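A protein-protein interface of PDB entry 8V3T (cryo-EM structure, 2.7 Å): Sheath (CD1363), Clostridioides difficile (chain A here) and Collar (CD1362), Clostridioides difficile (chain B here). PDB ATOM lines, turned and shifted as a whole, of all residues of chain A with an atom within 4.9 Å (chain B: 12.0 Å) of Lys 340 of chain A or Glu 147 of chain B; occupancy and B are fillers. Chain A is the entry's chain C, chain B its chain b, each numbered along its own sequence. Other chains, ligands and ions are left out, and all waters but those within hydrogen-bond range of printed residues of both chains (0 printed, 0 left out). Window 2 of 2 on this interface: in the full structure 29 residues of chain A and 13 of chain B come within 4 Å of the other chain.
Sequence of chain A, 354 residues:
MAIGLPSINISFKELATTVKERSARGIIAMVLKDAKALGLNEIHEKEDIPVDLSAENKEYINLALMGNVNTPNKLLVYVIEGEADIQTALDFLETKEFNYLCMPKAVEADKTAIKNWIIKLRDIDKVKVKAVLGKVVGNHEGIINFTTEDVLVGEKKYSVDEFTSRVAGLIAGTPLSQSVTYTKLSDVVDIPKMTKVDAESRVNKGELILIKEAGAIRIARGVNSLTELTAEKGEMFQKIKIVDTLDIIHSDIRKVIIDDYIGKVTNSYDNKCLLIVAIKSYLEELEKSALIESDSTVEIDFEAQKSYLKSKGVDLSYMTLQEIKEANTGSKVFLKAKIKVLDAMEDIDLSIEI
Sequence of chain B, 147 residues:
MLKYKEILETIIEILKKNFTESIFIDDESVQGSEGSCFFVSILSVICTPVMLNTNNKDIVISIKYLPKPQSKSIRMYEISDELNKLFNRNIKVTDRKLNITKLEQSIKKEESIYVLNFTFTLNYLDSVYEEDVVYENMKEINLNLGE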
ATOM      1  N   MET A 236      29.560 -20.971  -8.260  1.00  0.00           N
ATOM      2  CA  MET A 236      28.432 -20.710  -7.373  1.00  0.00           C
ATOM      3  C   MET A 236      27.121 -20.498  -8.118  1.00  0.00           C
ATOM      4  O   MET A 236      26.053 -20.653  -7.518  1.00  0.00           O
ATOM      5  CB  MET A 236      28.730 -19.494  -6.494  1.00  0.00           C
ATOM      6  CG  MET A 236      28.437 -18.159  -7.157  1.00  0.00           C
ATOM      7  SD  MET A 236      28.814 -16.750  -6.098  1.00  0.00           S
ATOM      8  CE  MET A 236      30.321 -17.313  -5.310  1.00  0.00           C
ATOM      9  N   LEU A 246      19.402 -14.563  -4.620  1.00  0.00           N
ATOM     10  CA  LEU A 246      19.784 -13.336  -5.311  1.00  0.00           C
ATOM     11  C   LEU A 246      18.584 -12.705  -6.010  1.00  0.00           C
ATOM     12  O   LEU A 246      18.367 -11.488  -5.922  1.00  0.00           O
ATOM     13  CB  LEU A 246      20.893 -13.633  -6.317  1.00  0.00           C
ATOM     14  CG  LEU A 246      22.298 -13.839  -5.748  1.00  0.00           C
ATOM     15  CD1 LEU A 246      23.217 -14.444  -6.796  1.00  0.00           C
ATOM     16  CD2 LEU A 246      22.873 -12.544  -5.215  1.00  0.00           C
ATOM     17  N   ILE A 292      22.347 -13.268   4.446  1.00  0.00           N
ATOM     18  CA  ILE A 292      23.557 -13.079   3.660  1.00  0.00           C
ATOM     19  C   ILE A 292      24.710 -12.786   4.608  1.00  0.00           C
ATOM     20  O   ILE A 292      24.515 -12.388   5.759  1.00  0.00           O
ATOM     21  CB  ILE A 292      23.414 -11.942   2.626  1.00  0.00           C
ATOM     22  CG1 ILE A 292      23.206 -10.603   3.335  1.00  0.00           C
ATOM     23  CG2 ILE A 292      22.275 -12.230   1.666  1.00  0.00           C
ATOM     24  CD1 ILE A 292      23.239  -9.410   2.412  1.00  0.00           C
ATOM     25  N   GLU A 293      25.926 -12.993   4.111  1.00  0.00           N
ATOM     26  CA  GLU A 293      27.107 -12.698   4.903  1.00  0.00           C
ATOM     27  C   GLU A 293      27.277 -11.190   5.067  1.00  0.00           C
ATOM     28  O   GLU A 293      26.778 -10.387   4.276  1.00  0.00           O
ATOM     29  CB  GLU A 293      28.353 -13.308   4.262  1.00  0.00           C
ATOM     30  CG  GLU A 293      28.421 -14.827   4.359  1.00  0.00           C
ATOM     31  CD  GLU A 293      27.846 -15.360   5.659  1.00  0.00           C
ATOM     32  OE1 GLU A 293      28.560 -15.335   6.684  1.00  0.00           O
ATOM     33  OE2 GLU A 293      26.682 -15.814   5.657  1.00  0.00           O
ATOM     34  N   LYS A 338      27.318  -5.403  -3.736  1.00  0.00           N
ATOM     35  CA  LYS A 338      28.153  -6.588  -3.579  1.00  0.00           C
ATOM     36  C   LYS A 338      27.723  -7.312  -2.313  1.00  0.00           C
ATOM     37  O   LYS A 338      27.816  -6.751  -1.218  1.00  0.00           O
ATOM     38  CB  LYS A 338      29.631  -6.197  -3.499  1.00  0.00           C
ATOM     39  CG  LYS A 338      30.136  -5.434  -4.720  1.00  0.00           C
ATOM     40  CD  LYS A 338      30.242  -6.292  -5.963  1.00  0.00           C
ATOM     41  CE  LYS A 338      31.128  -7.494  -5.738  1.00  0.00           C
ATOM     42  NZ  LYS A 338      31.204  -8.344  -6.956  1.00  0.00           N
ATOM     43  N   ILE A 339      27.255  -8.554  -2.456  1.00  0.00           N
ATOM     44  CA  ILE A 339      26.800  -9.362  -1.328  1.00  0.00           C
ATOM     45  C   ILE A 339      27.395 -10.760  -1.448  1.00  0.00           C
ATOM     46  O   ILE A 339      27.937 -11.143  -2.484  1.00  0.00           O
ATOM     47  CB  ILE A 339      25.261  -9.446  -1.234  1.00  0.00           C
ATOM     48  CG1 ILE A 339      24.705 -10.345  -2.335  1.00  0.00           C
ATOM     49  CG2 ILE A 339      24.629  -8.062  -1.292  1.00  0.00           C
ATOM     50  CD1 ILE A 339      23.331 -10.879  -2.031  1.00  0.00           C
ATOM     51  N   LYS A 340      27.290 -11.524  -0.361  1.00  0.00           N
ATOM     52  CA  LYS A 340      27.844 -12.869  -0.283  1.00  0.00           C
ATOM     53  C   LYS A 340      26.811 -13.829   0.287  1.00  0.00           C
ATOM     54  O   LYS A 340      26.114 -13.503   1.250  1.00  0.00           O
ATOM     55  CB  LYS A 340      29.106 -12.895   0.584  1.00  0.00           C
ATOM     56  CG  LYS A 340      30.022 -14.072   0.311  1.00  0.00           C
ATOM     57  CD  LYS A 340      31.203 -13.663  -0.549  1.00  0.00           C
ATOM     58  CE  LYS A 340      32.217 -14.790  -0.649  1.00  0.00           C
ATOM     59  NZ  LYS A 340      33.422 -14.388  -1.425  1.00  0.00           N
ATOM     60  N   VAL A 341      26.723 -15.019  -0.309  1.00  0.00           N
ATOM     61  CA  VAL A 341      25.802 -16.061   0.129  1.00  0.00           C
ATOM     62  C   VAL A 341      26.588 -17.346   0.355  1.00  0.00           C
ATOM     63  O   VAL A 341      27.658 -17.552  -0.226  1.00  0.00           O
ATOM     64  CB  VAL A 341      24.661 -16.296  -0.890  1.00  0.00           C
ATOM     65  CG1 VAL A 341      23.435 -16.866  -0.195  1.00  0.00           C
ATOM     66  CG2 VAL A 341      24.310 -15.010  -1.619  1.00  0.00           C
ATOM     67  N   LEU A 342      26.049 -18.215   1.208  1.00  0.00           N
ATOM     68  CA  LEU A 342      26.679 -19.481   1.548  1.00  0.00           C
ATOM     69  C   LEU A 342      25.788 -20.644   1.129  1.00  0.00           C
ATOM     70  O   LEU A 342      24.560 -20.532   1.115  1.00  0.00           O
ATOM     71  CB  LEU A 342      26.971 -19.578   3.050  1.00  0.00           C
ATOM     72  CG  LEU A 342      28.040 -18.652   3.628  1.00  0.00           C
ATOM     73  CD1 LEU A 342      28.212 -18.913   5.115  1.00  0.00           C
ATOM     74  CD2 LEU A 342      29.358 -18.822   2.897  1.00  0.00           C
ATOM     75  N   LEU B 143      20.423  -1.551 -11.269  1.00  0.00           N
ATOM     76  CA  LEU B 143      21.249  -2.025 -10.167  1.00  0.00           C
ATOM     77  C   LEU B 143      21.596  -3.489 -10.394  1.00  0.00           C
ATOM     78  O   LEU B 143      20.708  -4.306 -10.653  1.00  0.00           O
ATOM     79  CB  LEU B 143      20.534  -1.840  -8.823  1.00  0.00           C
ATOM     80  CG  LEU B 143      20.926  -2.740  -7.649  1.00  0.00           C
ATOM     81  CD1 LEU B 143      20.985  -1.929  -6.371  1.00  0.00           C
ATOM     82  CD2 LEU B 143      19.934  -3.879  -7.488  1.00  0.00           C
ATOM     83  N   ASN B 144      22.884  -3.813 -10.303  1.00  0.00           N
ATOM     84  CA  ASN B 144      23.364  -5.185 -10.411  1.00  0.00           C
ATOM     85  C   ASN B 144      24.061  -5.577  -9.115  1.00  0.00           C
ATOM     86  O   ASN B 144      24.977  -4.884  -8.660  1.00  0.00           O
ATOM     87  CB  ASN B 144      24.293  -5.358 -11.617  1.00  0.00           C
ATOM     88  CG  ASN B 144      25.505  -4.453 -11.568  1.00  0.00           C
ATOM     89  OD1 ASN B 144      25.527  -3.460 -10.843  1.00  0.00           O
ATOM     90  ND2 ASN B 144      26.532  -4.798 -12.336  1.00  0.00           N
ATOM     91  N   LEU B 145      23.621  -6.679  -8.520  1.00  0.00           N
ATOM     92  CA  LEU B 145      24.139  -7.147  -7.236  1.00  0.00           C
ATOM     93  C   LEU B 145      25.071  -8.336  -7.472  1.00  0.00           C
ATOM     94  O   LEU B 145      24.634  -9.429  -7.839  1.00  0.00           O
ATOM     95  CB  LEU B 145      22.987  -7.448  -6.279  1.00  0.00           C
ATOM     96  CG  LEU B 145      21.676  -8.119  -6.717  1.00  0.00           C
ATOM     97  CD1 LEU B 145      21.772  -9.619  -6.928  1.00  0.00           C
ATOM     98  CD2 LEU B 145      20.575  -7.791  -5.716  1.00  0.00           C
ATOM     99  N   GLY B 146      26.369  -8.099  -7.285  1.00  0.00           N
ATOM    100  CA  GLY B 146      27.364  -9.111  -7.572  1.00  0.00           C
ATOM    101  C   GLY B 146      27.489 -10.155  -6.479  1.00  0.00           C
ATOM    102  O   GLY B 146      27.040  -9.978  -5.346  1.00  0.00           O
ATOM    103  N   GLU B 147      28.143 -11.258  -6.842  1.00  0.00           N
ATOM    104  CA  GLU B 147      28.313 -12.437  -5.987  1.00  0.00           C
ATOM    105  C   GLU B 147      27.031 -12.825  -5.254  1.00  0.00           C
ATOM    106  O   GLU B 147      27.010 -13.795  -4.496  1.00  0.00           O
ATOM    107  CB  GLU B 147      29.439 -12.228  -4.968  1.00  0.00           C
ATOM    108  CG  GLU B 147      30.654 -11.464  -5.466  1.00  0.00           C
ATOM    109  CD  GLU B 147      31.475 -10.890  -4.323  1.00  0.00           C
ATOM    110  OE1 GLU B 147      31.216 -11.263  -3.158  1.00  0.00           O
ATOM    111  OE2 GLU B 147      32.395 -10.089  -4.584  1.00  0.00           O
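The side-chain carboxylate (OE2) of Glu 147 of chain B is in salt-bridge range of the side-chain amino group (NZ) of Lys 338 of chain A (3.2 Å).
O of Gly 146 of chain B sits at hydrogen-bond distance from N of Ile 339 of chain A.
The backbone carbonyl oxygen of Ile 339 of chain A sits close to the side-chain carboxylate of Glu 147 of chain B (3.3 Å).
N of Glu 293 of chain A lies within hydrogen-bond range of O of Lys 340 of chain A (2.9 Å).
Among the printed residues, merely in contact across the chains: Met 236 of chain A with Glu 147 of chain B (3.8 Å), Leu 246 of chain A with Leu 145 of chain B (3.6 Å), Lys 338 of chain A with Gly 146 of chain B (3.96 Å) and Lys 340 of chain A with Glu 147 of chain B (3.5 Å).
Lys 340 of chain A touches just one residue of chain B: Glu 147 (3.5 Å).
Glu 147 of chain B touches just these residues of chain A: Met 236, Lys 338, Ile 339 and Lys 340.
No residue of chain B comes within 4 Å of Glu 293 of chain A.
Of chain B, only Gly 146 and Glu 147 come within 4 Å of Lys 338 of chain A.
Leu 342 of chain A touches none of the printed residues of chain B.
Printed residues of chain B within 4 Å of Leu 246 of chain A: Leu 145 (3.6 Å).
Of the printed residues of chain B, Met 236 of chain A touches Glu 147 (3.8 Å).
Asn 144 of chain B touches none of the printed residues of chain A.
Leu 143 of chain B touches none of the printed residues of chain A.
The nearest residue of chain A that does not touch Glu 147 of chain B is Val 341 of chain A (4.1 Å).
The nearest printed residue of chain A that does not touch Leu 145 of chain B is Lys 338 of chain A (5.0 Å).
Of the 9 printed residues of chain A, 5 touch a printed residue of chain B.
Hydrophobic or aromatic side chains of chain A that line the printed part of chain B: Met 236, Leu 246 and Ile 339.
Among the printed residues, 7 pairs touch across the chains.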
